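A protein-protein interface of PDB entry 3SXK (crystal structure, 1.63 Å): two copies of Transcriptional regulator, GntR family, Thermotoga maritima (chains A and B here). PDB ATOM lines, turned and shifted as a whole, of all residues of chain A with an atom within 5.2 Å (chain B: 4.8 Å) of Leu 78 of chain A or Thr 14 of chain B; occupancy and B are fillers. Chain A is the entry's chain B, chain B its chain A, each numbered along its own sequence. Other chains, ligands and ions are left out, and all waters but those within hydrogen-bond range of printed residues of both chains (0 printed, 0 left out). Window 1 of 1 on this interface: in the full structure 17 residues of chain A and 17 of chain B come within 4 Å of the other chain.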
ATOM      1  N   MET A  18       1.788   9.708  18.241  1.00  0.00           N
ATOM      2  CA  MET A  18       1.675   9.617  19.677  1.00  0.00           C
ATOM      3  C   MET A  18       2.818   8.831  20.332  1.00  0.00           C
ATOM      4  O   MET A  18       3.446   9.281  21.301  1.00  0.00           O
ATOM      5  CB  MET A  18       0.319   9.005  20.057  1.00  0.00           C
ATOM      6  CG  MET A  18      -0.848   9.891  19.652  1.00  0.00           C
ATOM      7  SD  MET A  18      -2.471   9.205  20.128  1.00  0.00           S
ATOM      8  CE  MET A  18      -2.397   9.544  21.811  1.00  0.00           C
ATOM      9  N   ASN A  72       1.039  11.767  31.077  1.00  0.00           N
ATOM     10  CA  ASN A  72       0.114  12.809  30.622  1.00  0.00           C
ATOM     11  C   ASN A  72      -1.254  12.191  30.471  1.00  0.00           C
ATOM     12  O   ASN A  72      -1.483  11.402  29.575  1.00  0.00           O
ATOM     13  CB  ASN A  72       0.621  13.410  29.319  1.00  0.00           C
ATOM     14  CG  ASN A  72      -0.317  14.444  28.742  1.00  0.00           C
ATOM     15  OD1 ASN A  72      -1.558  14.322  28.824  1.00  0.00           O
ATOM     16  ND2 ASN A  72       0.267  15.476  28.170  1.00  0.00           N
ATOM     17  N   GLU A  73      -2.186  12.483  31.396  1.00  0.00           N
ATOM     18  CA  GLU A  73      -3.437  11.753  31.378  1.00  0.00           C
ATOM     19  C   GLU A  73      -4.284  12.044  30.145  1.00  0.00           C
ATOM     20  O   GLU A  73      -5.083  11.190  29.738  1.00  0.00           O
ATOM     21  CB  GLU A  73      -4.240  12.011  32.672  1.00  0.00           C
ATOM     22  CG  GLU A  73      -3.535  11.532  33.937  1.00  0.00           C
ATOM     23  CD  GLU A  73      -3.405   9.991  34.050  1.00  0.00           C
ATOM     24  OE1 GLU A  73      -3.502   9.460  35.171  1.00  0.00           O
ATOM     25  OE2 GLU A  73      -3.209   9.308  33.036  1.00  0.00           O
ATOM     26  N   LEU A  74      -4.097  13.202  29.522  1.00  0.00           N
ATOM     27  CA  LEU A  74      -4.825  13.516  28.297  1.00  0.00           C
ATOM     28  C   LEU A  74      -4.320  12.613  27.162  1.00  0.00           C
ATOM     29  O   LEU A  74      -5.110  12.021  26.466  1.00  0.00           O
ATOM     30  CB  LEU A  74      -4.755  15.013  27.942  1.00  0.00           C
ATOM     31  CG  LEU A  74      -5.509  15.427  26.687  1.00  0.00           C
ATOM     32  CD1 LEU A  74      -6.976  15.032  26.752  1.00  0.00           C
ATOM     33  CD2 LEU A  74      -5.356  16.925  26.413  1.00  0.00           C
ATOM     34  N   ILE A  75      -3.008  12.498  27.019  1.00  0.00           N
ATOM     35  CA  ILE A  75      -2.440  11.609  25.979  1.00  0.00           C
ATOM     36  C   ILE A  75      -2.848  10.174  26.203  1.00  0.00           C
ATOM     37  O   ILE A  75      -3.240   9.469  25.255  1.00  0.00           O
ATOM     38  CB  ILE A  75      -0.906  11.782  25.877  1.00  0.00           C
ATOM     39  CG1 ILE A  75      -0.532  13.209  25.442  1.00  0.00           C
ATOM     40  CG2 ILE A  75      -0.334  10.785  24.879  1.00  0.00           C
ATOM     41  CD1 ILE A  75       0.970  13.505  25.359  1.00  0.00           C
ATOM     42  N   ILE A  76      -2.762   9.727  27.457  1.00  0.00           N
ATOM     43  CA  ILE A  76      -3.170   8.384  27.817  1.00  0.00           C
ATOM     44  C   ILE A  76      -4.643   8.134  27.474  1.00  0.00           C
ATOM     45  O   ILE A  76      -5.004   7.092  26.917  1.00  0.00           O
ATOM     46  CB  ILE A  76      -2.881   8.152  29.311  1.00  0.00           C
ATOM     47  CG1 ILE A  76      -1.389   8.128  29.560  1.00  0.00           C
ATOM     48  CG2 ILE A  76      -3.569   6.870  29.826  1.00  0.00           C
ATOM     49  CD1 ILE A  76      -0.931   8.299  31.062  1.00  0.00           C
ATOM     50  N   SER A  77      -5.519   9.096  27.776  1.00  0.00           N
ATOM     51  CA  SER A  77      -6.938   8.958  27.474  1.00  0.00           C
ATOM     52  C   SER A  77      -7.233   8.927  25.984  1.00  0.00           C
ATOM     53  O   SER A  77      -8.124   8.183  25.541  1.00  0.00           O
ATOM     54  CB  SER A  77      -7.811  10.042  28.176  1.00  0.00           C
ATOM     55  OG  SER A  77      -7.681  11.340  27.613  1.00  0.00           O
ATOM     56  N   LEU A  78      -6.509   9.735  25.216  1.00  0.00           N
ATOM     57  CA  LEU A  78      -6.700   9.781  23.772  1.00  0.00           C
ATOM     58  C   LEU A  78      -6.258   8.437  23.169  1.00  0.00           C
ATOM     59  O   LEU A  78      -6.929   7.937  22.279  1.00  0.00           O
ATOM     60  CB  LEU A  78      -5.943  10.937  23.147  1.00  0.00           C
ATOM     61  CG  LEU A  78      -6.475  12.355  23.425  1.00  0.00           C
ATOM     62  CD1 LEU A  78      -5.557  13.367  22.830  1.00  0.00           C
ATOM     63  CD2 LEU A  78      -7.884  12.561  22.880  1.00  0.00           C
ATOM     64  N   TYR A  79      -5.146   7.885  23.640  1.00  0.00           N
ATOM     65  CA  TYR A  79      -4.685   6.565  23.176  1.00  0.00           C
ATOM     66  C   TYR A  79      -5.692   5.476  23.527  1.00  0.00           C
ATOM     67  O   TYR A  79      -6.009   4.601  22.704  1.00  0.00           O
ATOM     68  CB  TYR A  79      -3.303   6.302  23.713  1.00  0.00           C
ATOM     69  CG  TYR A  79      -2.586   5.189  22.971  1.00  0.00           C
ATOM     70  CD1 TYR A  79      -1.936   5.439  21.776  1.00  0.00           C
ATOM     71  CD2 TYR A  79      -2.511   3.936  23.515  1.00  0.00           C
ATOM     72  CE1 TYR A  79      -1.255   4.427  21.104  1.00  0.00           C
ATOM     73  CE2 TYR A  79      -1.847   2.900  22.832  1.00  0.00           C
ATOM     74  CZ  TYR A  79      -1.238   3.169  21.647  1.00  0.00           C
ATOM     75  OH  TYR A  79      -0.566   2.138  21.015  1.00  0.00           O
ATOM     76  N   GLU A  80      -6.240   5.534  24.733  1.00  0.00           N
ATOM     77  CA  GLU A  80      -7.266   4.577  25.106  1.00  0.00           C
ATOM     78  C   GLU A  80      -8.517   4.740  24.249  1.00  0.00           C
ATOM     79  O   GLU A  80      -9.157   3.750  23.899  1.00  0.00           O
ATOM     80  CB  GLU A  80      -7.584   4.626  26.600  1.00  0.00           C
ATOM     81  CG  GLU A  80      -8.147   3.324  27.165  1.00  0.00           C
ATOM     82  CD  GLU A  80      -7.162   2.161  27.083  1.00  0.00           C
ATOM     83  OE1 GLU A  80      -6.002   2.337  27.530  1.00  0.00           O
ATOM     84  OE2 GLU A  80      -7.535   1.088  26.564  1.00  0.00           O
ATOM     85  N   LYS A  81      -8.864   5.975  23.890  1.00  0.00           N
ATOM     86  CA  LYS A  81     -10.032   6.220  23.042  1.00  0.00           C
ATOM     87  C   LYS A  81      -9.891   5.519  21.690  1.00  0.00           C
ATOM     88  O   LYS A  81     -10.873   5.011  21.152  1.00  0.00           O
ATOM     89  CB  LYS A  81     -10.215   7.727  22.796  1.00  0.00           C
ATOM     90  CG  LYS A  81     -11.454   8.031  21.938  1.00  0.00           C
ATOM     91  CD  LYS A  81     -11.467   9.446  21.339  1.00  0.00           C
ATOM     92  CE  LYS A  81     -12.439   9.541  20.136  1.00  0.00           C
ATOM     93  NZ  LYS A  81     -12.030   8.697  18.934  1.00  0.00           N
ATOM     94  N   ILE A  82      -8.683   5.538  21.133  1.00  0.00           N
ATOM     95  CA  ILE A  82      -8.474   5.007  19.792  1.00  0.00           C
ATOM     96  C   ILE A  82      -8.019   3.521  19.858  1.00  0.00           C
ATOM     97  O   ILE A  82      -7.782   2.897  18.833  1.00  0.00           O
ATOM     98  CB  ILE A  82      -7.443   5.818  18.940  1.00  0.00           C
ATOM     99  CG1 ILE A  82      -6.032   5.764  19.525  1.00  0.00           C
ATOM    100  CG2 ILE A  82      -7.929   7.282  18.779  1.00  0.00           C
ATOM    101  CD1 ILE A  82      -4.965   6.449  18.575  1.00  0.00           C
ATOM    102  N   GLU B  10      -0.542  19.457  30.613  1.00  0.00           N
ATOM    103  CA  GLU B  10      -0.937  18.304  29.786  1.00  0.00           C
ATOM    104  C   GLU B  10      -1.565  18.785  28.465  1.00  0.00           C
ATOM    105  O   GLU B  10      -1.373  18.145  27.387  1.00  0.00           O
ATOM    106  CB  GLU B  10      -1.932  17.414  30.506  1.00  0.00           C
ATOM    107  CG  GLU B  10      -1.373  16.570  31.618  1.00  0.00           C
ATOM    108  CD  GLU B  10      -2.442  15.653  32.181  1.00  0.00           C
ATOM    109  OE1 GLU B  10      -3.635  15.870  31.847  1.00  0.00           O
ATOM    110  OE2 GLU B  10      -2.110  14.812  33.019  1.00  0.00           O
ATOM    111  N   THR B  11      -2.321  19.879  28.545  1.00  0.00           N
ATOM    112  CA  THR B  11      -2.986  20.437  27.365  1.00  0.00           C
ATOM    113  C   THR B  11      -1.958  20.925  26.353  1.00  0.00           C
ATOM    114  O   THR B  11      -2.011  20.591  25.168  1.00  0.00           O
ATOM    115  CB  THR B  11      -3.923  21.603  27.741  1.00  0.00           C
ATOM    116  OG1 THR B  11      -4.856  21.128  28.693  1.00  0.00           O
ATOM    117  CG2 THR B  11      -4.682  22.083  26.555  1.00  0.00           C
ATOM    118  N   ILE B  12      -1.008  21.713  26.824  1.00  0.00           N
ATOM    119  CA  ILE B  12       0.009  22.254  25.929  1.00  0.00           C
ATOM    120  C   ILE B  12       0.913  21.165  25.352  1.00  0.00           C
ATOM    121  O   ILE B  12       1.246  21.198  24.161  1.00  0.00           O
ATOM    122  CB  ILE B  12       0.882  23.306  26.657  1.00  0.00           C
ATOM    123  CG1 ILE B  12       0.015  24.480  27.140  1.00  0.00           C
ATOM    124  CG2 ILE B  12       2.012  23.711  25.780  1.00  0.00           C
ATOM    125  CD1 ILE B  12      -0.624  25.255  26.040  1.00  0.00           C
ATOM    126  N   GLU B  13       1.300  20.194  26.179  1.00  0.00           N
ATOM    127  CA  GLU B  13       2.104  19.032  25.676  1.00  0.00           C
ATOM    128  C   GLU B  13       1.368  18.274  24.577  1.00  0.00           C
ATOM    129  O   GLU B  13       1.937  17.940  23.548  1.00  0.00           O
ATOM    130  CB  GLU B  13       2.494  18.106  26.805  1.00  0.00           C
ATOM    131  CG  GLU B  13       3.408  16.986  26.327  1.00  0.00           C
ATOM    132  CD  GLU B  13       3.893  16.059  27.429  1.00  0.00           C
ATOM    133  OE1 GLU B  13       3.111  15.737  28.347  1.00  0.00           O
ATOM    134  OE2 GLU B  13       5.079  15.681  27.385  1.00  0.00           O
ATOM    135  N   THR B  14       0.087  18.043  24.777  1.00  0.00           N
ATOM    136  CA  THR B  14      -0.719  17.407  23.746  1.00  0.00           C
ATOM    137  C   THR B  14      -0.734  18.194  22.450  1.00  0.00           C
ATOM    138  O   THR B  14      -0.632  17.611  21.354  1.00  0.00           O
ATOM    139  CB  THR B  14      -2.132  17.091  24.247  1.00  0.00           C
ATOM    140  OG1 THR B  14      -2.031  16.271  25.420  1.00  0.00           O
ATOM    141  CG2 THR B  14      -2.966  16.354  23.197  1.00  0.00           C
ATOM    142  N   ARG B  15      -0.891  19.502  22.540  1.00  0.00           N
ATOM    143  CA  ARG B  15      -0.858  20.386  21.372  1.00  0.00           C
ATOM    144  C   ARG B  15       0.490  20.334  20.688  1.00  0.00           C
ATOM    145  O   ARG B  15       0.549  20.283  19.443  1.00  0.00           O
ATOM    146  CB  ARG B  15      -1.159  21.835  21.780  1.00  0.00           C
ATOM    147  CG  ARG B  15      -2.586  22.035  22.252  1.00  0.00           C
ATOM    148  CD  ARG B  15      -2.867  23.508  22.543  1.00  0.00           C
ATOM    149  NE  ARG B  15      -2.864  24.317  21.338  1.00  0.00           N
ATOM    150  CZ  ARG B  15      -2.950  25.635  21.312  1.00  0.00           C
ATOM    151  NH1 ARG B  15      -3.127  26.314  22.438  1.00  0.00           N
ATOM    152  NH2 ARG B  15      -2.886  26.266  20.164  1.00  0.00           N
ATOM    153  N   ILE B  16       1.579  20.351  21.454  1.00  0.00           N
ATOM    154  CA  ILE B  16       2.908  20.264  20.837  1.00  0.00           C
ATOM    155  C   ILE B  16       3.021  18.943  20.066  1.00  0.00           C
ATOM    156  O   ILE B  16       3.418  18.921  18.884  1.00  0.00           O
ATOM    157  CB  ILE B  16       4.007  20.429  21.882  1.00  0.00           C
ATOM    158  CG1 ILE B  16       4.041  21.855  22.397  1.00  0.00           C
ATOM    159  CG2 ILE B  16       5.358  20.058  21.261  1.00  0.00           C
ATOM    160  CD1 ILE B  16       4.905  22.008  23.619  1.00  0.00           C
ATOM    161  N   MET B  17       2.649  17.845  20.709  1.00  0.00           N
ATOM    162  CA  MET B  17       2.619  16.537  20.042  1.00  0.00           C
ATOM    163  C   MET B  17       1.894  16.521  18.691  1.00  0.00           C
ATOM    164  O   MET B  17       2.457  16.056  17.667  1.00  0.00           O
ATOM    165  CB  MET B  17       2.018  15.492  20.983  1.00  0.00           C
ATOM    166  CG  MET B  17       1.872  14.072  20.388  1.00  0.00           C
ATOM    167  SD  MET B  17       1.057  12.925  21.463  1.00  0.00           S
ATOM    168  CE  MET B  17      -0.615  13.553  21.388  1.00  0.00           C
ATOM    169  N   MET B  18       0.675  17.042  18.686  1.00  0.00           N
ATOM    170  CA  MET B  18      -0.169  16.990  17.517  1.00  0.00           C
ATOM    171  C   MET B  18       0.205  18.013  16.445  1.00  0.00           C
ATOM    172  O   MET B  18       0.374  17.674  15.263  1.00  0.00           O
ATOM    173  CB  MET B  18      -1.638  17.090  17.901  1.00  0.00           C
ATOM    174  CG  MET B  18      -2.115  15.901  18.731  1.00  0.00           C
ATOM    175  SD  MET B  18      -3.827  16.066  19.216  1.00  0.00           S
ATOM    176  CE  MET B  18      -4.578  15.654  17.745  1.00  0.00           C
ATOM    177  N   LEU B  78      -9.500  13.895  16.732  1.00  0.00           N
ATOM    178  CA  LEU B  78      -8.963  13.933  18.090  1.00  0.00           C
ATOM    179  C   LEU B  78      -8.697  15.394  18.524  1.00  0.00           C
ATOM    180  O   LEU B  78      -8.928  15.743  19.672  1.00  0.00           O
ATOM    181  CB  LEU B  78      -7.671  13.125  18.194  1.00  0.00           C
ATOM    182  CG  LEU B  78      -7.816  11.606  18.067  1.00  0.00           C
ATOM    183  CD1 LEU B  78      -6.446  10.975  18.049  1.00  0.00           C
ATOM    184  CD2 LEU B  78      -8.619  11.032  19.213  1.00  0.00           C
ATOM    185  N   LYS B  81     -11.929  16.885  19.409  1.00  0.00           N
ATOM    186  CA  LYS B  81     -12.390  16.349  20.699  1.00  0.00           C
ATOM    187  C   LYS B  81     -11.798  17.178  21.850  1.00  0.00           C
ATOM    188  O   LYS B  81     -12.499  17.438  22.826  1.00  0.00           O
ATOM    189  CB  LYS B  81     -11.988  14.867  20.890  1.00  0.00           C
ATOM    190  CG  LYS B  81     -12.454  14.256  22.217  1.00  0.00           C
ATOM    191  CD  LYS B  81     -11.713  12.973  22.632  1.00  0.00           C
ATOM    192  CE  LYS B  81     -11.899  12.684  24.140  1.00  0.00           C
ATOM    193  NZ  LYS B  81     -11.171  13.654  25.069  1.00  0.00           N
ATOM    194  N   ILE B  82     -10.524  17.567  21.726  1.00  0.00           N
ATOM    195  CA  ILE B  82      -9.821  18.279  22.796  1.00  0.00           C
ATOM    196  C   ILE B  82      -9.961  19.837  22.666  1.00  0.00           C
ATOM    197  O   ILE B  82      -9.445  20.583  23.497  1.00  0.00           O
ATOM    198  CB  ILE B  82      -8.336  17.894  22.963  1.00  0.00           C
ATOM    199  CG1 ILE B  82      -7.495  18.273  21.743  1.00  0.00           C
ATOM    200  CG2 ILE B  82      -8.228  16.411  23.267  1.00  0.00           C
ATOM    201  CD1 ILE B  82      -5.967  18.108  21.978  1.00  0.00           C
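ND2 of Asn 72 of chain A is in hydrogen-bond range of O of Glu 10 of chain B (3.2 Å). The side-chain carboxylate (OE2) of Glu 10 of chain B sits at hydrogen-bond distance from the backbone NH (N) of Glu 73 of chain A, at 2.8 Å. The side-chain carboxylate of Glu 13 of chain B is in hydrogen-bond range of the side-chain amide nitrogen of Asn 72 of chain A (2.9 Å).
The side-chain hydroxyl (OG1) of Thr 14 of chain B sits at hydrogen-bond distance from the backbone carbonyl oxygen (O) of Glu 10 of chain B (2.8 Å). The side-chain amide oxygen (OD1) of Asn 72 of chain A sits at hydrogen-bond distance from the backbone NH (N) of Leu 74 of chain A, at 2.9 Å. The side-chain amide oxygen (OD1) of Asn 72 of chain A sits at hydrogen-bond distance from the backbone NH (N) of Ile 75 of chain A (2.9 Å). The side-chain hydroxyl (OG) of Ser 77 of chain A lies close to the backbone carbonyl oxygen (O) of Glu 73 of chain A, at 3.4 Å. The side-chain hydroxyl (OG) of Ser 77 of chain A sits at hydrogen-bond distance from the backbone carbonyl oxygen (O) of Leu 74 of chain A (2.9 Å).
Among the printed residues, pairs that only touch across the chains: Met 18 of chain A with Met 17 of chain B, Asn 72 of chain A with Thr 14 of chain B, Leu 74 of chain A with Glu 10 of chain B, Leu 74 of chain A with Thr 14 of chain B, Leu 74 of chain A with Ile 82 of chain B, Ile 75 of chain A with Thr 14 of chain B, Ile 75 of chain A with Met 17 of chain B, Leu 78 of chain A with Thr 14 of chain B, Leu 78 of chain A with Lys 81 of chain B, Leu 78 of chain A with Ile 82 of chain B, Lys 81 of chain A with Leu 78 of chain B, Lys 81 of chain A with Lys 81 of chain B and Ile 82 of chain A with Leu 78 of chain B.
Of the printed residues of chain B, Asn 72 of chain A touches Glu 10, Glu 13 and Thr 14. Ile 76 of chain A touches none of the printed residues of chain B. Of chain B, only Thr 14 (3.97 Å), Lys 81 (3.9 Å) and Ile 82 (3.9 Å) come within 4 Å of Leu 78 of chain A. Of the printed residues of chain B, Ile 82 of chain A touches Leu 78 (3.8 Å). Of chain A, only Asn 72, Leu 74, Ile 75 and Leu 78 come within 4 Å of Thr 14 of chain B. Arg 15 of chain B touches none of the printed residues of chain A. Of the printed residues of chain A, Met 17 of chain B touches Met 18 and Ile 75. Printed residues of chain A within 4 Å of Leu 78 of chain B: Lys 81 (3.9 Å) and Ile 82 (3.8 Å). The nearest residue of chain B that does not touch Leu 78 of chain A is Leu 78 of chain B (4.04 Å). The nearest printed residue of chain A that does not touch Thr 14 of chain B is Glu 73 of chain A (6.7 Å).
Of the 12 printed residues of chain A, 8 touch a printed residue of chain B. Hydrophobic or aromatic side chains of chain B that line the printed part of chain A: Met 17, Leu 78 and Ile 82. Among the printed residues, no Asp or Glu carboxylate lies within 4 Å of a Lys or Arg side-chain nitrogen of the other chain.
Leu 78 of chain A touches Lys 81 of chain B, and with the chains exchanged Lys 81 of chain A touches Leu 78 of chain B. Leu 78 of chain A touches Ile 82 of chain B, and with the chains exchanged Ile 82 of chain A touches Leu 78 of chain B. Lys 81 of chain B touches its own counterpart, Lys 81 of chain A.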
